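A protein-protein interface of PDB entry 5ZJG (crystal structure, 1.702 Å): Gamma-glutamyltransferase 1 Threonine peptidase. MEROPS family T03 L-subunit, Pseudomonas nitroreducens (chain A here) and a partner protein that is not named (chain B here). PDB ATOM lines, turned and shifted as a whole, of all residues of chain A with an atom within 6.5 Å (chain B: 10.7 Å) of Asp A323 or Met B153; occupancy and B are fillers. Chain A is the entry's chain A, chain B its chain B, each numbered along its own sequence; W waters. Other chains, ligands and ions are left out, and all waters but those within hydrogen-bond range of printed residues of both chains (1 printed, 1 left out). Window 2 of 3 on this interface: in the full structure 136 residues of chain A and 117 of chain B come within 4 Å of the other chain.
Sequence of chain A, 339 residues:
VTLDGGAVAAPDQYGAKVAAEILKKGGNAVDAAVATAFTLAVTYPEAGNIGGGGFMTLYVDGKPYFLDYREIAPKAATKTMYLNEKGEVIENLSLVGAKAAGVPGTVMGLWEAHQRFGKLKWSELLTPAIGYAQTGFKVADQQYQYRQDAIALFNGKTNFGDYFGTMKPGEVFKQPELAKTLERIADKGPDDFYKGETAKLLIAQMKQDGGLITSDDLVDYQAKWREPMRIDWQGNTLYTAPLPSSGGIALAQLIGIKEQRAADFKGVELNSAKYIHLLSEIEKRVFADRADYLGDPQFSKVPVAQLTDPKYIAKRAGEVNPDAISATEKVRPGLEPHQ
Of the printed residues of chain B, Ala A273 touches Val B146 (3.6 Å), Glu B149 (3.2 Å) and Leu B150 (3.6 Å). Printed residues of chain B within 4 Å of His A277: Met B153 and Tyr B155. No residue of chain B comes within 4 Å of Asn A321. No residue of chain B comes within 4 Å of Pro A322. Of chain B, only Met B153 comes within 4 Å of Asp A323. Printed residues of chain B within 4 Å of Ile A325: Asp B132 (3.2 Å), Met B153 (3.2 Å), Gly B154 (3.6 Å) and Tyr B155 (3.6 Å). Of the printed residues of chain A, Asp B132 touches Ile A325. Of the printed residues of chain A, Val B146 touches Ala A273. Met B153 touches just these residues of chain A: His A277, Asp A323, Ala A324 and Ile A325.
A ring nitrogen (NE2) of His A277 lies within hydrogen-bond range of the backbone carbonyl oxygen of Asn A321. A ring nitrogen (NE2) of His A277 sits close to the backbone carbonyl oxygen (O) of Ala A324, at 3.4 Å. The backbone NH (N) of Asp A323 lies within hydrogen-bond range of the side-chain amide oxygen (OD1) of Asn A321, 2.9 Å away. OD1 of Asn A321 lies within hydrogen-bond range of N of Ala A324. The backbone NH of Thr B156 lies within hydrogen-bond range of the backbone carbonyl oxygen of Asp B132. O of Leu B150 is in hydrogen-bond range of N of Tyr B155, at 3.1 Å.
The side-chain hydroxyl (OH) of Tyr B155 sits at hydrogen-bond distance from a ring nitrogen (ND1) of His A277, 2.8 Å away.
Printed residues of chain A that touch a printed residue of chain B: Ala A273, His A277, Asp A323, Ala A324 and Ile A325. Hydrophobic or aromatic side chains of chain A that line the printed part of chain B: Ala A273, His A277 and Ile A325. Of the 17 printed residues of chain B, 7 touch a printed residue of chain A. Hydrophobic or aromatic side chains of chain B that line the printed part of chain A: Val B146, Leu B150, Met B153 and Tyr B155. Among the printed residues, no Asp or Glu carboxylate lies within 4 Å of a Lys or Arg side-chain nitrogen of the other chain.
Among the printed residues, pairs that only touch across the chains: Ile A325 with Asp B132 (3.2 Å), Ile A325 with Met B153 (3.2 Å), Ala A273 with Glu B149 (3.2 Å), His A277 with Met B153 (3.5 Å), Ile A325 with Tyr B155 (3.6 Å), Ala A273 with Val B146 (3.6 Å), Ala A273 with Leu B150 (3.6 Å), Ile A325 with Gly B154 (3.6 Å), Asp A323 with Met B153 (3.8 Å) and Ala A324 with Met B153 (3.9 Å).
Water W1 bridges O of Met B153 (2.6 Å) and N of Ile A325 (3.1 Å).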
ATOM      1  N   ALA A 273       1.408  17.055  -1.438  1.00  0.00           N
ATOM      2  CA  ALA A 273       1.858  18.147  -0.575  1.00  0.00           C
ATOM      3  C   ALA A 273       0.940  19.358  -0.707  1.00  0.00           C
ATOM      4  O   ALA A 273       0.583  19.989   0.294  1.00  0.00           O
ATOM      5  CB  ALA A 273       3.302  18.534  -0.899  1.00  0.00           C
ATOM      6  N   LYS A 274       0.550  19.700  -1.938  1.00  0.00           N
ATOM      7  CA  LYS A 274      -0.370  20.815  -2.132  1.00  0.00           C
ATOM      8  C   LYS A 274      -1.695  20.580  -1.410  1.00  0.00           C
ATOM      9  O   LYS A 274      -2.234  21.504  -0.788  1.00  0.00           O
ATOM     10  CB  LYS A 274      -0.614  21.056  -3.621  1.00  0.00           C
ATOM     11  CG  LYS A 274      -1.687  22.106  -3.902  1.00  0.00           C
ATOM     12  CD  LYS A 274      -1.205  23.211  -4.835  1.00  0.00           C
ATOM     13  CE  LYS A 274      -2.167  24.385  -4.787  1.00  0.00           C
ATOM     14  NZ  LYS A 274      -2.276  25.098  -6.086  1.00  0.00           N
ATOM     15  N   HIS A 277      -1.037  21.020   2.292  1.00  0.00           N
ATOM     16  CA  HIS A 277      -0.801  22.434   2.563  1.00  0.00           C
ATOM     17  C   HIS A 277      -2.107  23.220   2.566  1.00  0.00           C
ATOM     18  O   HIS A 277      -2.342  24.046   3.459  1.00  0.00           O
ATOM     19  CB  HIS A 277       0.155  23.046   1.538  1.00  0.00           C
ATOM     20  CG  HIS A 277       0.118  24.542   1.547  1.00  0.00           C
ATOM     21  ND1 HIS A 277       0.589  25.284   2.612  1.00  0.00           N
ATOM     22  CD2 HIS A 277      -0.417  25.430   0.677  1.00  0.00           C
ATOM     23  CE1 HIS A 277       0.389  26.566   2.371  1.00  0.00           C
ATOM     24  NE2 HIS A 277      -0.224  26.683   1.209  1.00  0.00           N
ATOM     25  N   LEU A 278      -2.978  22.965   1.589  1.00  0.00           N
ATOM     26  CA  LEU A 278      -4.243  23.685   1.524  1.00  0.00           C
ATOM     27  C   LEU A 278      -5.110  23.381   2.738  1.00  0.00           C
ATOM     28  O   LEU A 278      -5.693  24.296   3.331  1.00  0.00           O
ATOM     29  CB  LEU A 278      -4.999  23.324   0.247  1.00  0.00           C
ATOM     30  CG  LEU A 278      -4.439  23.940  -1.039  1.00  0.00           C
ATOM     31  CD1 LEU A 278      -5.100  23.295  -2.253  1.00  0.00           C
ATOM     32  CD2 LEU A 278      -4.645  25.427  -1.065  1.00  0.00           C
ATOM     33  N   VAL A 320      -6.608  31.983   2.665  1.00  0.00           N
ATOM     34  CA  VAL A 320      -5.817  30.801   2.387  1.00  0.00           C
ATOM     35  C   VAL A 320      -4.751  31.153   1.363  1.00  0.00           C
ATOM     36  O   VAL A 320      -5.035  31.779   0.333  1.00  0.00           O
ATOM     37  CB  VAL A 320      -6.727  29.661   1.908  1.00  0.00           C
ATOM     38  CG1 VAL A 320      -5.914  28.509   1.350  1.00  0.00           C
ATOM     39  CG2 VAL A 320      -7.590  29.179   3.078  1.00  0.00           C
ATOM     40  N   ASN A 321      -3.511  30.745   1.638  1.00  0.00           N
ATOM     41  CA  ASN A 321      -2.411  30.956   0.712  1.00  0.00           C
ATOM     42  C   ASN A 321      -2.095  29.636   0.010  1.00  0.00           C
ATOM     43  O   ASN A 321      -1.486  28.743   0.619  1.00  0.00           O
ATOM     44  CB  ASN A 321      -1.179  31.485   1.454  1.00  0.00           C
ATOM     45  CG  ASN A 321      -0.059  31.904   0.506  1.00  0.00           C
ATOM     46  OD1 ASN A 321       0.115  31.320  -0.549  1.00  0.00           O
ATOM     47  ND2 ASN A 321       0.701  32.922   0.893  1.00  0.00           N
ATOM     48  N   PRO A 322      -2.489  29.442  -1.253  1.00  0.00           N
ATOM     49  CA  PRO A 322      -2.263  28.136  -1.888  1.00  0.00           C
ATOM     50  C   PRO A 322      -0.805  27.831  -2.186  1.00  0.00           C
ATOM     51  O   PRO A 322      -0.497  26.684  -2.528  1.00  0.00           O
ATOM     52  CB  PRO A 322      -3.072  28.233  -3.187  1.00  0.00           C
ATOM     53  CG  PRO A 322      -3.077  29.686  -3.501  1.00  0.00           C
ATOM     54  CD  PRO A 322      -3.137  30.394  -2.171  1.00  0.00           C
ATOM     55  N   ASP A 323       0.096  28.811  -2.085  1.00  0.00           N
ATOM     56  CA  ASP A 323       1.460  28.658  -2.572  1.00  0.00           C
ATOM     57  C   ASP A 323       2.523  28.664  -1.482  1.00  0.00           C
ATOM     58  O   ASP A 323       3.627  28.164  -1.724  1.00  0.00           O
ATOM     59  CB  ASP A 323       1.780  29.775  -3.577  1.00  0.00           C
ATOM     60  CG  ASP A 323       0.972  29.649  -4.855  1.00  0.00           C
ATOM     61  OD1 ASP A 323       0.875  28.522  -5.383  1.00  0.00           O
ATOM     62  OD2 ASP A 323       0.422  30.672  -5.316  1.00  0.00           O
ATOM     63  N   ALA A 324       2.223  29.200  -0.299  1.00  0.00           N
ATOM     64  CA  ALA A 324       3.190  29.232   0.789  1.00  0.00           C
ATOM     65  C   ALA A 324       2.446  29.257   2.112  1.00  0.00           C
ATOM     66  O   ALA A 324       1.264  29.606   2.166  1.00  0.00           O
ATOM     67  CB  ALA A 324       4.124  30.448   0.707  1.00  0.00           C
ATOM     68  N   ILE A 325       3.177  28.912   3.177  1.00  0.00           N
ATOM     69  CA  ILE A 325       2.626  28.901   4.536  1.00  0.00           C
ATOM     70  C   ILE A 325       2.354  30.324   5.003  1.00  0.00           C
ATOM     71  O   ILE A 325       3.240  31.192   4.961  1.00  0.00           O
ATOM     72  CB  ILE A 325       3.596  28.206   5.505  1.00  0.00           C
ATOM     73  CG1 ILE A 325       3.836  26.759   5.105  1.00  0.00           C
ATOM     74  CG2 ILE A 325       3.059  28.272   6.943  1.00  0.00           C
ATOM     75  CD1 ILE A 325       4.866  26.030   5.968  1.00  0.00           C
ATOM     76  N   LYS B 131       3.064  25.985  16.041  1.00  0.00           N
ATOM     77  CA  LYS B 131       3.289  26.695  14.788  1.00  0.00           C
ATOM     78  C   LYS B 131       3.734  25.745  13.692  1.00  0.00           C
ATOM     79  O   LYS B 131       4.671  24.962  13.872  1.00  0.00           O
ATOM     80  CB  LYS B 131       4.341  27.793  15.004  1.00  0.00           C
ATOM     81  CG  LYS B 131       4.858  28.468  13.727  1.00  0.00           C
ATOM     82  CD  LYS B 131       5.939  29.532  14.059  1.00  0.00           C
ATOM     83  CE  LYS B 131       6.505  30.236  12.815  1.00  0.00           C
ATOM     84  NZ  LYS B 131       7.602  31.217  13.151  1.00  0.00           N
ATOM     85  N   ASP B 132       3.022  25.792  12.570  1.00  0.00           N
ATOM     86  CA  ASP B 132       3.443  25.121  11.333  1.00  0.00           C
ATOM     87  C   ASP B 132       3.814  23.654  11.554  1.00  0.00           C
ATOM     88  O   ASP B 132       4.738  23.128  10.930  1.00  0.00           O
ATOM     89  CB  ASP B 132       4.612  25.869  10.697  1.00  0.00           C
ATOM     90  CG  ASP B 132       4.223  27.242  10.236  1.00  0.00           C
ATOM     91  OD1 ASP B 132       3.015  27.468  10.026  1.00  0.00           O
ATOM     92  OD2 ASP B 132       5.122  28.097  10.075  1.00  0.00           O
ATOM     93  N   THR B 133       3.089  22.982  12.441  1.00  0.00           N
ATOM     94  CA  THR B 133       3.342  21.583  12.765  1.00  0.00           C
ATOM     95  C   THR B 133       2.202  20.743  12.201  1.00  0.00           C
ATOM     96  O   THR B 133       1.032  21.001  12.495  1.00  0.00           O
ATOM     97  CB  THR B 133       3.478  21.395  14.280  1.00  0.00           C
ATOM     98  OG1 THR B 133       4.644  22.098  14.738  1.00  0.00           O
ATOM     99  CG2 THR B 133       3.633  19.936  14.648  1.00  0.00           C
ATOM    100  N   ILE B 134       2.547  19.777  11.349  1.00  0.00           N
ATOM    101  CA  ILE B 134       1.592  18.812  10.817  1.00  0.00           C
ATOM    102  C   ILE B 134       1.855  17.483  11.501  1.00  0.00           C
ATOM    103  O   ILE B 134       2.987  16.977  11.477  1.00  0.00           O
ATOM    104  CB  ILE B 134       1.702  18.657   9.290  1.00  0.00           C
ATOM    105  CG1 ILE B 134       1.414  19.974   8.571  1.00  0.00           C
ATOM    106  CG2 ILE B 134       0.710  17.592   8.803  1.00  0.00           C
ATOM    107  CD1 ILE B 134       1.860  19.965   7.069  1.00  0.00           C
ATOM    108  N   LYS B 145       8.405  11.852  -1.128  1.00  0.00           N
ATOM    109  CA  LYS B 145       8.326  13.128  -1.835  1.00  0.00           C
ATOM    110  C   LYS B 145       7.462  14.134  -1.075  1.00  0.00           C
ATOM    111  O   LYS B 145       7.872  15.280  -0.855  1.00  0.00           O
ATOM    112  CB  LYS B 145       7.783  12.901  -3.248  1.00  0.00           C
ATOM    113  CG  LYS B 145       7.507  14.178  -4.021  1.00  0.00           C
ATOM    114  N   VAL B 146       6.254  13.726  -0.680  1.00  0.00           N
ATOM    115  CA  VAL B 146       5.323  14.647  -0.031  1.00  0.00           C
ATOM    116  C   VAL B 146       5.930  15.212   1.251  1.00  0.00           C
ATOM    117  O   VAL B 146       5.811  16.411   1.532  1.00  0.00           O
ATOM    118  CB  VAL B 146       3.978  13.939   0.239  1.00  0.00           C
ATOM    119  CG1 VAL B 146       2.993  14.865   0.944  1.00  0.00           C
ATOM    120  CG2 VAL B 146       3.361  13.438  -1.060  1.00  0.00           C
ATOM    121  N   ALA B 147       6.597  14.365   2.043  1.00  0.00           N
ATOM    122  CA  ALA B 147       7.191  14.839   3.293  1.00  0.00           C
ATOM    123  C   ALA B 147       8.333  15.814   3.034  1.00  0.00           C
ATOM    124  O   ALA B 147       8.453  16.838   3.720  1.00  0.00           O
ATOM    125  CB  ALA B 147       7.685  13.657   4.124  1.00  0.00           C
ATOM    126  N   ASP B 148       9.194  15.512   2.054  1.00  0.00           N
ATOM    127  CA  ASP B 148      10.225  16.471   1.677  1.00  0.00           C
ATOM    128  C   ASP B 148       9.606  17.783   1.201  1.00  0.00           C
ATOM    129  O   ASP B 148      10.089  18.863   1.548  1.00  0.00           O
ATOM    130  CB  ASP B 148      11.125  15.887   0.583  1.00  0.00           C
ATOM    131  CG  ASP B 148      11.963  14.702   1.061  1.00  0.00           C
ATOM    132  OD1 ASP B 148      12.176  14.553   2.281  1.00  0.00           O
ATOM    133  OD2 ASP B 148      12.423  13.917   0.201  1.00  0.00           O
ATOM    134  N   GLU B 149       8.554  17.715   0.384  1.00  0.00           N
ATOM    135  CA  GLU B 149       7.942  18.941  -0.125  1.00  0.00           C
ATOM    136  C   GLU B 149       7.394  19.787   1.013  1.00  0.00           C
ATOM    137  O   GLU B 149       7.586  21.007   1.050  1.00  0.00           O
ATOM    138  CB  GLU B 149       6.824  18.610  -1.113  1.00  0.00           C
ATOM    139  CG  GLU B 149       7.300  18.414  -2.556  1.00  0.00           C
ATOM    140  CD  GLU B 149       6.203  17.906  -3.479  1.00  0.00           C
ATOM    141  OE1 GLU B 149       5.316  17.172  -3.008  1.00  0.00           O
ATOM    142  OE2 GLU B 149       6.240  18.221  -4.693  1.00  0.00           O
ATOM    143  N   LEU B 150       6.682  19.153   1.944  1.00  0.00           N
ATOM    144  CA  LEU B 150       6.117  19.901   3.061  1.00  0.00           C
ATOM    145  C   LEU B 150       7.219  20.509   3.916  1.00  0.00           C
ATOM    146  O   LEU B 150       7.136  21.677   4.311  1.00  0.00           O
ATOM    147  CB  LEU B 150       5.215  18.986   3.892  1.00  0.00           C
ATOM    148  CG  LEU B 150       3.905  18.576   3.202  1.00  0.00           C
ATOM    149  CD1 LEU B 150       3.238  17.420   3.942  1.00  0.00           C
ATOM    150  CD2 LEU B 150       2.928  19.744   3.044  1.00  0.00           C
ATOM    151  N   LYS B 151       8.262  19.731   4.213  1.00  0.00           N
ATOM    152  CA  LYS B 151       9.387  20.264   4.972  1.00  0.00           C
ATOM    153  C   LYS B 151      10.059  21.408   4.223  1.00  0.00           C
ATOM    154  O   LYS B 151      10.450  22.412   4.829  1.00  0.00           O
ATOM    155  CB  LYS B 151      10.407  19.161   5.263  1.00  0.00           C
ATOM    156  CG  LYS B 151       9.961  18.116   6.289  1.00  0.00           C
ATOM    157  CD  LYS B 151      10.971  16.967   6.335  1.00  0.00           C
ATOM    158  CE  LYS B 151      10.704  16.013   7.491  1.00  0.00           C
ATOM    159  NZ  LYS B 151      11.895  15.167   7.784  1.00  0.00           N
ATOM    160  N   ALA B 152      10.208  21.271   2.904  1.00  0.00           N
ATOM    161  CA  ALA B 152      10.784  22.355   2.113  1.00  0.00           C
ATOM    162  C   ALA B 152       9.940  23.619   2.218  1.00  0.00           C
ATOM    163  O   ALA B 152      10.474  24.731   2.132  1.00  0.00           O
ATOM    164  CB  ALA B 152      10.921  21.925   0.652  1.00  0.00           C
ATOM    165  N   MET B 153       8.627  23.464   2.413  1.00  0.00           N
ATOM    166  CA  MET B 153       7.742  24.607   2.606  1.00  0.00           C
ATOM    167  C   MET B 153       7.924  25.254   3.969  1.00  0.00           C
ATOM    168  O   MET B 153       7.478  26.392   4.162  1.00  0.00           O
ATOM    169  CB  MET B 153       6.277  24.190   2.463  1.00  0.00           C
ATOM    170  CG  MET B 153       5.878  23.720   1.080  1.00  0.00           C
ATOM    171  SD  MET B 153       4.096  23.612   0.933  1.00  0.00           S
ATOM    172  CE  MET B 153       3.599  25.316   0.806  1.00  0.00           C
ATOM    173  N   GLY B 154       8.562  24.562   4.911  1.00  0.00           N
ATOM    174  CA  GLY B 154       8.746  25.072   6.254  1.00  0.00           C
ATOM    175  C   GLY B 154       7.851  24.438   7.292  1.00  0.00           C
ATOM    176  O   GLY B 154       7.782  24.939   8.419  1.00  0.00           O
ATOM    177  N   TYR B 155       7.151  23.368   6.946  1.00  0.00           N
ATOM    178  CA  TYR B 155       6.384  22.633   7.927  1.00  0.00           C
ATOM    179  C   TYR B 155       7.295  21.746   8.755  1.00  0.00           C
ATOM    180  O   TYR B 155       8.294  21.213   8.270  1.00  0.00           O
ATOM    181  CB  TYR B 155       5.332  21.755   7.251  1.00  0.00           C
ATOM    182  CG  TYR B 155       4.135  22.507   6.746  1.00  0.00           C
ATOM    183  CD1 TYR B 155       3.231  23.078   7.628  1.00  0.00           C
ATOM    184  CD2 TYR B 155       3.898  22.632   5.390  1.00  0.00           C
ATOM    185  CE1 TYR B 155       2.116  23.754   7.164  1.00  0.00           C
ATOM    186  CE2 TYR B 155       2.792  23.305   4.918  1.00  0.00           C
ATOM    187  CZ  TYR B 155       1.900  23.859   5.802  1.00  0.00           C
ATOM    188  OH  TYR B 155       0.804  24.526   5.306  1.00  0.00           O
ATOM    189  N   THR B 156       6.927  21.578  10.014  1.00  0.00           N
ATOM    190  CA  THR B 156       7.510  20.562  10.873  1.00  0.00           C
ATOM    191  C   THR B 156       6.564  19.372  10.898  1.00  0.00           C
ATOM    192  O   THR B 156       5.371  19.537  11.170  1.00  0.00           O
ATOM    193  CB  THR B 156       7.721  21.102  12.290  1.00  0.00           C
ATOM    194  OG1 THR B 156       8.669  22.177  12.254  1.00  0.00           O
ATOM    195  CG2 THR B 156       8.219  19.999  13.223  1.00  0.00           C
ATOM    196  N   LEU B 157       7.087  18.182  10.610  1.00  0.00           N
ATOM    197  CA  LEU B 157       6.301  16.955  10.644  1.00  0.00           C
ATOM    198  C   LEU B 157       6.632  16.158  11.895  1.00  0.00           C
ATOM    199  O   LEU B 157       7.807  15.970  12.226  1.00  0.00           O
ATOM    200  CB  LEU B 157       6.567  16.106   9.400  1.00  0.00           C
ATOM    201  CG  LEU B 157       6.604  16.905   8.101  1.00  0.00           C
ATOM    202  CD1 LEU B 157       6.823  15.978   6.910  1.00  0.00           C
ATOM    203  CD2 LEU B 157       5.336  17.720   7.928  1.00  0.00           C
HETATM  204  O   HOH W   1       6.138  28.213   2.840  1.00  0.00           O
